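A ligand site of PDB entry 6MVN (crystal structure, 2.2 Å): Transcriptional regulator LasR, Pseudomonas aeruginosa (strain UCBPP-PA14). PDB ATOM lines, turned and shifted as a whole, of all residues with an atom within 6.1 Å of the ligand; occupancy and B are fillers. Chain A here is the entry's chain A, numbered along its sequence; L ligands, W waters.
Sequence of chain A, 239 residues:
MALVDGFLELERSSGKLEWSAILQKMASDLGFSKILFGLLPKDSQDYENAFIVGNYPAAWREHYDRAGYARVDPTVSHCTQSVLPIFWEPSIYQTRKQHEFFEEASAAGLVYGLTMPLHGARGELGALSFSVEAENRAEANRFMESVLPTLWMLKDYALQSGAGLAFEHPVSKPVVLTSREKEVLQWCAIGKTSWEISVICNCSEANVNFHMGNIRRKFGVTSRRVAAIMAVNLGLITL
Leu 36 touches the ligand. Gly 38 touches the ligand (C to C13, 3.7 Å). Leu 39 touches the ligand (N to C13, 3.9 Å). Tyr 47 touches the ligand. Ala 50 touches the ligand (CB to C12, 3.6 Å). Ile 52 touches the ligand (CD1 to C10, 3.6 Å). NH2 of Arg 61 touches C9 of the ligand, at 3.7 Å. Tyr 64 touches the ligand (OH to C8, 3.4 Å). Val 76 touches the ligand (CG2 to C8, 3.9 Å). CZ2 of Trp 88 touches C1 of the ligand, at 3.6 Å. OH of Tyr 93 touches C4 of the ligand, 3.4 Å away. Phe 101 touches the ligand (CE1 to O2, 3.8 Å). CB of Ala 105 touches O2 of the ligand, at 3.5 Å. CD1 of Leu 110 touches O1 of the ligand, 3.7 Å away. O of Leu 125 touches C14 of the ligand, at 3.95 Å. Gly 126 touches the ligand. Hydrophobic or aromatic side chains that line the ligand: Leu 36, Tyr 47, Ala 50, Ile 52, Tyr 56, Trp 60, Tyr 64, Val 76, Trp 88, Phe 101, Ala 105 and Leu 110. 21 residues have an atom within 4 Å of the ligand: Leu 36, Gly 38, Leu 39, Tyr 47, Ala 50, Ile 52, Tyr 56, Trp 60, Arg 61, Tyr 64, Asp 73, Thr 75, Val 76, Trp 88, Tyr 93, Phe 101, Ala 105, Leu 110, Leu 125, Gly 126 and Ser 129.
Water W1 bridges NH2 of Arg 61 (2.8 Å) and O4 of the ligand (2.8 Å).
OG of Ser 129 is in hydrogen-bond range of OG1 of Thr 115 (2.9 Å). OD2 of Asp 73 sits at hydrogen-bond distance from OH of Tyr 64. N of Leu 110 is in hydrogen-bond range of O of Ala 105. The indole nitrogen (NE1) of Trp 88 is in hydrogen-bond range of the side-chain hydroxyl (OG1) of Thr 115, at 2.9 Å. The guanidinium group (NH1) of Arg 61 is in salt-bridge range of the side-chain carboxylate (OD2) of Asp 65, at 3.2 Å. N of Ala 127 sits at hydrogen-bond distance from O of Gly 38 (2.9 Å). O of Phe 51 sits at hydrogen-bond distance from N of Leu 39, at 2.8 Å. The backbone NH (N) of Leu 40 is in hydrogen-bond range of the backbone carbonyl oxygen (O) of Leu 125.
O3 of the ligand is in hydrogen-bond range of OG of Ser 129, 2.6 Å away. N1 of the ligand is in hydrogen-bond range of OD2 of Asp 73 (2.7 Å). NE1 of Trp 60 is in hydrogen-bond range of O1 of the ligand (2.8 Å). OH of Tyr 56 sits at hydrogen-bond distance from O3 of the ligand, at 2.8 Å. OG1 of Thr 75 lies close to N1 of the ligand, at 3.4 Å.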
ATOM      1  N   LEU A  36       0.456  -2.628 -37.397  1.00  0.00           N
ATOM      2  CA  LEU A  36      -0.424  -2.099 -36.399  1.00  0.00           C
ATOM      3  C   LEU A  36      -0.242  -0.589 -36.363  1.00  0.00           C
ATOM      4  O   LEU A  36       0.877  -0.097 -36.224  1.00  0.00           O
ATOM      5  CB  LEU A  36      -0.143  -2.711 -35.020  1.00  0.00           C
ATOM      6  CG  LEU A  36      -1.072  -2.102 -33.956  1.00  0.00           C
ATOM      7  CD1 LEU A  36      -1.675  -3.177 -33.073  1.00  0.00           C
ATOM      8  CD2 LEU A  36      -0.357  -1.048 -33.127  1.00  0.00           C
ATOM      9  N   GLY A  38      -1.720   2.352 -34.018  1.00  0.00           N
ATOM     10  CA  GLY A  38      -2.430   2.529 -32.779  1.00  0.00           C
ATOM     11  C   GLY A  38      -2.284   3.942 -32.238  1.00  0.00           C
ATOM     12  O   GLY A  38      -1.190   4.490 -32.223  1.00  0.00           O
ATOM     13  N   LEU A  39      -3.391   4.519 -31.782  1.00  0.00           N
ATOM     14  CA  LEU A  39      -3.392   5.927 -31.422  1.00  0.00           C
ATOM     15  C   LEU A  39      -4.239   6.223 -30.182  1.00  0.00           C
ATOM     16  O   LEU A  39      -5.361   5.689 -30.018  1.00  0.00           O
ATOM     17  CB  LEU A  39      -3.877   6.759 -32.595  1.00  0.00           C
ATOM     18  CG  LEU A  39      -3.391   8.209 -32.648  1.00  0.00           C
ATOM     19  CD1 LEU A  39      -1.882   8.255 -32.577  1.00  0.00           C
ATOM     20  CD2 LEU A  39      -3.886   8.880 -33.911  1.00  0.00           C
ATOM     21  N   LEU A  40      -3.687   7.061 -29.321  1.00  0.00           N
ATOM     22  CA  LEU A  40      -4.324   7.552 -28.106  1.00  0.00           C
ATOM     23  C   LEU A  40      -4.305   9.065 -28.076  1.00  0.00           C
ATOM     24  O   LEU A  40      -3.350   9.684 -28.559  1.00  0.00           O
ATOM     25  CB  LEU A  40      -3.607   7.021 -26.865  1.00  0.00           C
ATOM     26  CG  LEU A  40      -3.959   5.638 -26.350  1.00  0.00           C
ATOM     27  CD1 LEU A  40      -3.187   5.371 -25.077  1.00  0.00           C
ATOM     28  CD2 LEU A  40      -5.468   5.525 -26.134  1.00  0.00           C
ATOM     29  N   TYR A  47      -4.697   2.366 -22.869  1.00  0.00           N
ATOM     30  CA  TYR A  47      -4.126   1.602 -23.980  1.00  0.00           C
ATOM     31  C   TYR A  47      -5.062   0.522 -24.541  1.00  0.00           C
ATOM     32  O   TYR A  47      -5.024   0.209 -25.723  1.00  0.00           O
ATOM     33  CB  TYR A  47      -2.818   0.964 -23.549  1.00  0.00           C
ATOM     34  CG  TYR A  47      -1.755   1.973 -23.160  1.00  0.00           C
ATOM     35  CD1 TYR A  47      -1.116   2.735 -24.123  1.00  0.00           C
ATOM     36  CD2 TYR A  47      -1.400   2.147 -21.825  1.00  0.00           C
ATOM     37  CE1 TYR A  47      -0.138   3.657 -23.765  1.00  0.00           C
ATOM     38  CE2 TYR A  47      -0.438   3.069 -21.461  1.00  0.00           C
ATOM     39  CZ  TYR A  47       0.198   3.820 -22.434  1.00  0.00           C
ATOM     40  OH  TYR A  47       1.170   4.734 -22.076  1.00  0.00           O
ATOM     41  N   ALA A  50      -7.288   2.082 -27.200  1.00  0.00           N
ATOM     42  CA  ALA A  50      -6.673   2.862 -28.259  1.00  0.00           C
ATOM     43  C   ALA A  50      -7.397   2.636 -29.567  1.00  0.00           C
ATOM     44  O   ALA A  50      -8.074   1.625 -29.745  1.00  0.00           O
ATOM     45  CB  ALA A  50      -5.201   2.502 -28.401  1.00  0.00           C
ATOM     46  N   PHE A  51      -7.266   3.586 -30.482  1.00  0.00           N
ATOM     47  CA  PHE A  51      -7.667   3.396 -31.859  1.00  0.00           C
ATOM     48  C   PHE A  51      -6.638   2.465 -32.497  1.00  0.00           C
ATOM     49  O   PHE A  51      -5.456   2.772 -32.475  1.00  0.00           O
ATOM     50  CB  PHE A  51      -7.734   4.743 -32.598  1.00  0.00           C
ATOM     51  CG  PHE A  51      -7.934   4.624 -34.087  1.00  0.00           C
ATOM     52  CD1 PHE A  51      -8.990   3.892 -34.619  1.00  0.00           C
ATOM     53  CD2 PHE A  51      -7.077   5.270 -34.964  1.00  0.00           C
ATOM     54  CE1 PHE A  51      -9.167   3.803 -35.990  1.00  0.00           C
ATOM     55  CE2 PHE A  51      -7.262   5.187 -36.339  1.00  0.00           C
ATOM     56  CZ  PHE A  51      -8.293   4.463 -36.854  1.00  0.00           C
ATOM     57  N   ILE A  52      -7.096   1.350 -33.058  1.00  0.00           N
ATOM     58  CA  ILE A  52      -6.202   0.353 -33.639  1.00  0.00           C
ATOM     59  C   ILE A  52      -6.608  -0.014 -35.049  1.00  0.00           C
ATOM     60  O   ILE A  52      -7.762  -0.346 -35.301  1.00  0.00           O
ATOM     61  CB  ILE A  52      -6.181  -0.965 -32.802  1.00  0.00           C
ATOM     62  CG1 ILE A  52      -5.914  -0.698 -31.320  1.00  0.00           C
ATOM     63  CG2 ILE A  52      -5.172  -1.956 -33.372  1.00  0.00           C
ATOM     64  CD1 ILE A  52      -4.469  -0.336 -31.008  1.00  0.00           C
ATOM     65  N   TYR A  56      -2.879  -7.394 -37.110  1.00  0.00           N
ATOM     66  CA  TYR A  56      -2.292  -8.232 -36.064  1.00  0.00           C
ATOM     67  C   TYR A  56      -3.273  -9.363 -35.751  1.00  0.00           C
ATOM     68  O   TYR A  56      -4.475  -9.180 -35.898  1.00  0.00           O
ATOM     69  CB  TYR A  56      -2.011  -7.412 -34.805  1.00  0.00           C
ATOM     70  CG  TYR A  56      -0.664  -6.735 -34.779  1.00  0.00           C
ATOM     71  CD1 TYR A  56       0.029  -6.453 -35.957  1.00  0.00           C
ATOM     72  CD2 TYR A  56      -0.064  -6.385 -33.583  1.00  0.00           C
ATOM     73  CE1 TYR A  56       1.273  -5.850 -35.928  1.00  0.00           C
ATOM     74  CE2 TYR A  56       1.170  -5.800 -33.532  1.00  0.00           C
ATOM     75  CZ  TYR A  56       1.831  -5.521 -34.699  1.00  0.00           C
ATOM     76  OH  TYR A  56       3.074  -4.906 -34.619  1.00  0.00           O
ATOM     77  N   TRP A  60      -3.835 -12.241 -30.455  1.00  0.00           N
ATOM     78  CA  TRP A  60      -2.755 -11.454 -29.862  1.00  0.00           C
ATOM     79  C   TRP A  60      -3.273 -10.144 -29.321  1.00  0.00           C
ATOM     80  O   TRP A  60      -2.996  -9.791 -28.179  1.00  0.00           O
ATOM     81  CB  TRP A  60      -1.646 -11.183 -30.883  1.00  0.00           C
ATOM     82  CG  TRP A  60      -0.535 -10.319 -30.326  1.00  0.00           C
ATOM     83  CD1 TRP A  60      -0.095  -9.131 -30.822  1.00  0.00           C
ATOM     84  CD2 TRP A  60       0.276 -10.598 -29.166  1.00  0.00           C
ATOM     85  NE1 TRP A  60       0.947  -8.661 -30.077  1.00  0.00           N
ATOM     86  CE2 TRP A  60       1.196  -9.534 -29.052  1.00  0.00           C
ATOM     87  CE3 TRP A  60       0.323 -11.633 -28.235  1.00  0.00           C
ATOM     88  CZ2 TRP A  60       2.142  -9.477 -28.028  1.00  0.00           C
ATOM     89  CZ3 TRP A  60       1.264 -11.573 -27.224  1.00  0.00           C
ATOM     90  CH2 TRP A  60       2.159 -10.503 -27.129  1.00  0.00           C
ATOM     91  N   ARG A  61      -4.035  -9.422 -30.143  1.00  0.00           N
ATOM     92  CA  ARG A  61      -4.606  -8.146 -29.717  1.00  0.00           C
ATOM     93  C   ARG A  61      -5.425  -8.283 -28.433  1.00  0.00           C
ATOM     94  O   ARG A  61      -5.305  -7.466 -27.528  1.00  0.00           O
ATOM     95  CB  ARG A  61      -5.451  -7.542 -30.840  1.00  0.00           C
ATOM     96  CG  ARG A  61      -4.632  -7.128 -32.068  1.00  0.00           C
ATOM     97  CD  ARG A  61      -4.308  -5.629 -32.083  1.00  0.00           C
ATOM     98  NE  ARG A  61      -3.439  -5.207 -30.979  1.00  0.00           N
ATOM     99  CZ  ARG A  61      -3.880  -4.666 -29.841  1.00  0.00           C
ATOM    100  NH1 ARG A  61      -5.183  -4.483 -29.659  1.00  0.00           N
ATOM    101  NH2 ARG A  61      -3.026  -4.314 -28.909  1.00  0.00           N
ATOM    102  N   TYR A  64      -3.146  -9.270 -25.416  1.00  0.00           N
ATOM    103  CA  TYR A  64      -2.347  -8.078 -25.139  1.00  0.00           C
ATOM    104  C   TYR A  64      -3.093  -7.104 -24.244  1.00  0.00           C
ATOM    105  O   TYR A  64      -2.592  -6.672 -23.199  1.00  0.00           O
ATOM    106  CB  TYR A  64      -1.976  -7.403 -26.463  1.00  0.00           C
ATOM    107  CG  TYR A  64      -0.983  -6.241 -26.450  1.00  0.00           C
ATOM    108  CD1 TYR A  64      -1.338  -4.980 -25.978  1.00  0.00           C
ATOM    109  CD2 TYR A  64       0.281  -6.400 -27.019  1.00  0.00           C
ATOM    110  CE1 TYR A  64      -0.432  -3.913 -26.037  1.00  0.00           C
ATOM    111  CE2 TYR A  64       1.183  -5.356 -27.075  1.00  0.00           C
ATOM    112  CZ  TYR A  64       0.829  -4.120 -26.588  1.00  0.00           C
ATOM    113  OH  TYR A  64       1.748  -3.086 -26.670  1.00  0.00           O
ATOM    114  N   ASP A  65      -4.296  -6.745 -24.678  1.00  0.00           N
ATOM    115  CA  ASP A  65      -5.143  -5.820 -23.932  1.00  0.00           C
ATOM    116  C   ASP A  65      -5.594  -6.416 -22.593  1.00  0.00           C
ATOM    117  O   ASP A  65      -5.535  -5.741 -21.564  1.00  0.00           O
ATOM    118  CB  ASP A  65      -6.361  -5.441 -24.787  1.00  0.00           C
ATOM    119  CG  ASP A  65      -5.982  -4.605 -25.989  1.00  0.00           C
ATOM    120  OD1 ASP A  65      -4.865  -4.036 -25.991  1.00  0.00           O
ATOM    121  OD2 ASP A  65      -6.822  -4.482 -26.907  1.00  0.00           O
ATOM    122  N   ALA A  70       0.590  -3.407 -22.690  1.00  0.00           N
ATOM    123  CA  ALA A  70       1.063  -2.074 -23.054  1.00  0.00           C
ATOM    124  C   ALA A  70       2.037  -1.528 -22.025  1.00  0.00           C
ATOM    125  O   ALA A  70       2.889  -0.709 -22.363  1.00  0.00           O
ATOM    126  CB  ALA A  70      -0.107  -1.138 -23.200  1.00  0.00           C
ATOM    127  N   ASP A  73       5.188  -4.177 -23.066  1.00  0.00           N
ATOM    128  CA  ASP A  73       5.745  -4.042 -24.407  1.00  0.00           C
ATOM    129  C   ASP A  73       6.839  -2.984 -24.408  1.00  0.00           C
ATOM    130  O   ASP A  73       6.556  -1.803 -24.176  1.00  0.00           O
ATOM    131  CB  ASP A  73       4.615  -3.683 -25.380  1.00  0.00           C
ATOM    132  CG  ASP A  73       5.028  -3.773 -26.839  1.00  0.00           C
ATOM    133  OD1 ASP A  73       6.254  -3.767 -27.142  1.00  0.00           O
ATOM    134  OD2 ASP A  73       4.085  -3.860 -27.677  1.00  0.00           O
ATOM    135  N   THR A  75       8.247  -1.673 -26.777  1.00  0.00           N
ATOM    136  CA  THR A  75       8.104  -0.690 -27.843  1.00  0.00           C
ATOM    137  C   THR A  75       7.184   0.424 -27.375  1.00  0.00           C
ATOM    138  O   THR A  75       7.306   1.562 -27.809  1.00  0.00           O
ATOM    139  CB  THR A  75       7.580  -1.307 -29.170  1.00  0.00           C
ATOM    140  OG1 THR A  75       6.236  -1.785 -28.997  1.00  0.00           O
ATOM    141  CG2 THR A  75       8.495  -2.455 -29.590  1.00  0.00           C
ATOM    142  N   VAL A  76       6.284   0.120 -26.445  1.00  0.00           N
ATOM    143  CA  VAL A  76       5.314   1.137 -26.049  1.00  0.00           C
ATOM    144  C   VAL A  76       5.923   2.127 -25.072  1.00  0.00           C
ATOM    145  O   VAL A  76       5.766   3.329 -25.261  1.00  0.00           O
ATOM    146  CB  VAL A  76       4.031   0.522 -25.453  1.00  0.00           C
ATOM    147  CG1 VAL A  76       3.109   1.624 -24.941  1.00  0.00           C
ATOM    148  CG2 VAL A  76       3.322  -0.326 -26.507  1.00  0.00           C
ATOM    149  N   TRP A  88      12.755  -4.440 -33.385  1.00  0.00           N
ATOM    150  CA  TRP A  88      12.440  -5.518 -32.459  1.00  0.00           C
ATOM    151  C   TRP A  88      13.639  -6.462 -32.303  1.00  0.00           C
ATOM    152  O   TRP A  88      13.533  -7.655 -32.575  1.00  0.00           O
ATOM    153  CB  TRP A  88      11.216  -6.306 -32.926  1.00  0.00           C
ATOM    154  CG  TRP A  88       9.950  -5.484 -33.154  1.00  0.00           C
ATOM    155  CD1 TRP A  88       9.759  -4.161 -32.878  1.00  0.00           C
ATOM    156  CD2 TRP A  88       8.720  -5.963 -33.710  1.00  0.00           C
ATOM    157  NE1 TRP A  88       8.485  -3.779 -33.231  1.00  0.00           N
ATOM    158  CE2 TRP A  88       7.823  -4.877 -33.739  1.00  0.00           C
ATOM    159  CE3 TRP A  88       8.276  -7.211 -34.189  1.00  0.00           C
ATOM    160  CZ2 TRP A  88       6.510  -4.986 -34.226  1.00  0.00           C
ATOM    161  CZ3 TRP A  88       6.969  -7.324 -34.665  1.00  0.00           C
ATOM    162  CH2 TRP A  88       6.101  -6.223 -34.677  1.00  0.00           C
ATOM    163  N   ILE A  92      15.865  -5.593 -26.787  1.00  0.00           N
ATOM    164  CA  ILE A  92      14.870  -4.660 -26.256  1.00  0.00           C
ATOM    165  C   ILE A  92      13.993  -5.405 -25.251  1.00  0.00           C
ATOM    166  O   ILE A  92      13.268  -4.795 -24.454  1.00  0.00           O
ATOM    167  CB  ILE A  92      13.983  -4.004 -27.348  1.00  0.00           C
ATOM    168  CG1 ILE A  92      13.006  -5.005 -27.989  1.00  0.00           C
ATOM    169  CG2 ILE A  92      14.836  -3.278 -28.389  1.00  0.00           C
ATOM    170  CD1 ILE A  92      11.886  -4.330 -28.804  1.00  0.00           C
ATOM    171  N   TYR A  93      14.070  -6.728 -25.286  1.00  0.00           N
ATOM    172  CA  TYR A  93      13.307  -7.549 -24.370  1.00  0.00           C
ATOM    173  C   TYR A  93      14.162  -7.896 -23.153  1.00  0.00           C
ATOM    174  O   TYR A  93      14.831  -8.923 -23.129  1.00  0.00           O
ATOM    175  CB  TYR A  93      12.804  -8.800 -25.079  1.00  0.00           C
ATOM    176  CG  TYR A  93      11.918  -8.481 -26.269  1.00  0.00           C
ATOM    177  CD1 TYR A  93      10.646  -7.932 -26.079  1.00  0.00           C
ATOM    178  CD2 TYR A  93      12.329  -8.732 -27.562  1.00  0.00           C
ATOM    179  CE1 TYR A  93       9.831  -7.641 -27.147  1.00  0.00           C
ATOM    180  CE2 TYR A  93      11.506  -8.447 -28.653  1.00  0.00           C
ATOM    181  CZ  TYR A  93      10.259  -7.902 -28.434  1.00  0.00           C
ATOM    182  OH  TYR A  93       9.428  -7.612 -29.496  1.00  0.00           O
ATOM    183  N   PHE A 101       6.808 -11.963 -22.876  1.00  0.00           N
ATOM    184  CA  PHE A 101       6.146 -11.171 -23.915  1.00  0.00           C
ATOM    185  C   PHE A 101       6.640 -11.585 -25.303  1.00  0.00           C
ATOM    186  O   PHE A 101       5.842 -11.854 -26.202  1.00  0.00           O
ATOM    187  CB  PHE A 101       6.423  -9.670 -23.690  1.00  0.00           C
ATOM    188  CG  PHE A 101       5.846  -8.766 -24.744  1.00  0.00           C
ATOM    189  CD1 PHE A 101       6.556  -8.509 -25.913  1.00  0.00           C
ATOM    190  CD2 PHE A 101       4.606  -8.189 -24.582  1.00  0.00           C
ATOM    191  CE1 PHE A 101       6.024  -7.686 -26.897  1.00  0.00           C
ATOM    192  CE2 PHE A 101       4.073  -7.366 -25.567  1.00  0.00           C
ATOM    193  CZ  PHE A 101       4.796  -7.118 -26.719  1.00  0.00           C
ATOM    194  N   ALA A 105       4.698 -13.180 -28.262  1.00  0.00           N
ATOM    195  CA  ALA A 105       4.586 -12.443 -29.530  1.00  0.00           C
ATOM    196  C   ALA A 105       5.093 -13.296 -30.697  1.00  0.00           C
ATOM    197  O   ALA A 105       4.549 -13.225 -31.793  1.00  0.00           O
ATOM    198  CB  ALA A 105       5.333 -11.114 -29.483  1.00  0.00           C
ATOM    199  N   LEU A 110       4.920 -12.566 -34.544  1.00  0.00           N
ATOM    200  CA  LEU A 110       5.506 -11.236 -34.450  1.00  0.00           C
ATOM    201  C   LEU A 110       6.938 -11.270 -33.932  1.00  0.00           C
ATOM    202  O   LEU A 110       7.199 -10.930 -32.772  1.00  0.00           O
ATOM    203  CB  LEU A 110       4.629 -10.330 -33.571  1.00  0.00           C
ATOM    204  CG  LEU A 110       3.256 -10.044 -34.180  1.00  0.00           C
ATOM    205  CD1 LEU A 110       2.366  -9.278 -33.196  1.00  0.00           C
ATOM    206  CD2 LEU A 110       3.423  -9.279 -35.486  1.00  0.00           C
ATOM    207  N   VAL A 111       7.874 -11.658 -34.801  1.00  0.00           N
ATOM    208  CA  VAL A 111       9.259 -11.852 -34.374  1.00  0.00           C
ATOM    209  C   VAL A 111      10.160 -10.712 -34.819  1.00  0.00           C
ATOM    210  O   VAL A 111      10.894 -10.130 -34.017  1.00  0.00           O
ATOM    211  CB  VAL A 111       9.828 -13.184 -34.918  1.00  0.00           C
ATOM    212  CG1 VAL A 111      11.233 -13.431 -34.349  1.00  0.00           C
ATOM    213  CG2 VAL A 111       8.897 -14.325 -34.588  1.00  0.00           C
ATOM    214  N   LEU A 114       9.840  -3.463 -36.558  1.00  0.00           N
ATOM    215  CA  LEU A 114      10.229  -2.230 -35.912  1.00  0.00           C
ATOM    216  C   LEU A 114       8.982  -1.446 -35.609  1.00  0.00           C
ATOM    217  O   LEU A 114       7.911  -1.731 -36.163  1.00  0.00           O
ATOM    218  CB  LEU A 114      11.188  -1.411 -36.779  1.00  0.00           C
ATOM    219  CG  LEU A 114      10.648  -0.614 -37.973  1.00  0.00           C
ATOM    220  CD1 LEU A 114      11.756   0.265 -38.543  1.00  0.00           C
ATOM    221  CD2 LEU A 114      10.167  -1.556 -39.049  1.00  0.00           C
ATOM    222  N   THR A 115       9.118  -0.482 -34.715  1.00  0.00           N
ATOM    223  CA  THR A 115       8.012   0.386 -34.333  1.00  0.00           C
ATOM    224  C   THR A 115       8.438   1.830 -34.434  1.00  0.00           C
ATOM    225  O   THR A 115       9.494   2.210 -33.902  1.00  0.00           O
ATOM    226  CB  THR A 115       7.549   0.087 -32.903  1.00  0.00           C
ATOM    227  OG1 THR A 115       7.134  -1.279 -32.823  1.00  0.00           O
ATOM    228  CG2 THR A 115       6.402   1.019 -32.502  1.00  0.00           C
ATOM    229  N   LEU A 125      -0.614  10.329 -28.856  1.00  0.00           N
ATOM    230  CA  LEU A 125       0.458   9.374 -28.661  1.00  0.00           C
ATOM    231  C   LEU A 125       0.079   8.113 -29.436  1.00  0.00           C
ATOM    232  O   LEU A 125      -1.090   7.724 -29.439  1.00  0.00           O
ATOM    233  CB  LEU A 125       0.650   9.050 -27.179  1.00  0.00           C
ATOM    234  CG  LEU A 125       1.373   7.749 -26.846  1.00  0.00           C
ATOM    235  CD1 LEU A 125       2.866   7.887 -27.167  1.00  0.00           C
ATOM    236  CD2 LEU A 125       1.182   7.396 -25.389  1.00  0.00           C
ATOM    237  N   GLY A 126       1.054   7.474 -30.079  1.00  0.00           N
ATOM    238  CA  GLY A 126       0.766   6.246 -30.770  1.00  0.00           C
ATOM    239  C   GLY A 126       1.953   5.483 -31.295  1.00  0.00           C
ATOM    240  O   GLY A 126       3.106   5.803 -30.999  1.00  0.00           O
ATOM    241  N   ALA A 127       1.685   4.462 -32.091  1.00  0.00           N
ATOM    242  CA  ALA A 127       2.741   3.645 -32.668  1.00  0.00           C
ATOM    243  C   ALA A 127       2.351   3.156 -34.040  1.00  0.00           C
ATOM    244  O   ALA A 127       1.172   2.866 -34.287  1.00  0.00           O
ATOM    245  CB  ALA A 127       3.046   2.458 -31.770  1.00  0.00           C
ATOM    246  N   SER A 129       3.757   0.066 -36.157  1.00  0.00           N
ATOM    247  CA  SER A 129       4.625  -1.096 -36.187  1.00  0.00           C
ATOM    248  C   SER A 129       4.495  -1.799 -37.518  1.00  0.00           C
ATOM    249  O   SER A 129       3.411  -1.857 -38.096  1.00  0.00           O
ATOM    250  CB  SER A 129       4.270  -2.079 -35.068  1.00  0.00           C
ATOM    251  OG  SER A 129       4.377  -1.468 -33.801  1.00  0.00           O
HETATM  252  C1  LIG L   1       4.966  -5.448 -31.025  1.00  0.00           C
HETATM  253  C2  LIG L   1       6.346  -5.918 -30.550  1.00  0.00           C
HETATM  254  C3  LIG L   1       4.126  -6.675 -30.684  1.00  0.00           C
HETATM  255  O1  LIG L   1       2.941  -6.814 -30.546  1.00  0.00           O
HETATM  256  O2  LIG L   1       4.909  -7.784 -30.515  1.00  0.00           O
HETATM  257  C4  LIG L   1       6.275  -7.427 -30.755  1.00  0.00           C
HETATM  258  N1  LIG L   1       4.437  -4.329 -30.314  1.00  0.00           N
HETATM  259  C5  LIG L   1       3.766  -3.320 -31.035  1.00  0.00           C
HETATM  260  O3  LIG L   1       3.610  -3.402 -32.263  1.00  0.00           O
HETATM  261  C6  LIG L   1       3.210  -2.171 -30.274  1.00  0.00           C
HETATM  262  C7  LIG L   1       1.736  -2.406 -30.004  1.00  0.00           C
HETATM  263  O4  LIG L   1       1.243  -3.480 -30.265  1.00  0.00           O
HETATM  264  C8  LIG L   1       0.939  -1.282 -29.416  1.00  0.00           C
HETATM  265  C9  LIG L   1      -0.529  -1.630 -29.135  1.00  0.00           C
HETATM  266  C10 LIG L   1      -1.369  -0.365 -29.157  1.00  0.00           C
HETATM  267  C11 LIG L   1      -0.818   0.653 -28.181  1.00  0.00           C
HETATM  268  C12 LIG L   1      -1.741   1.835 -27.959  1.00  0.00           C
HETATM  269  C13 LIG L   1      -1.354   3.032 -28.801  1.00  0.00           C
HETATM  270  C14 LIG L   1      -0.582   4.073 -28.006  1.00  0.00           C
HETATM  271  O   HOH W   1      -0.748  -5.468 -30.066  1.00  0.00           O
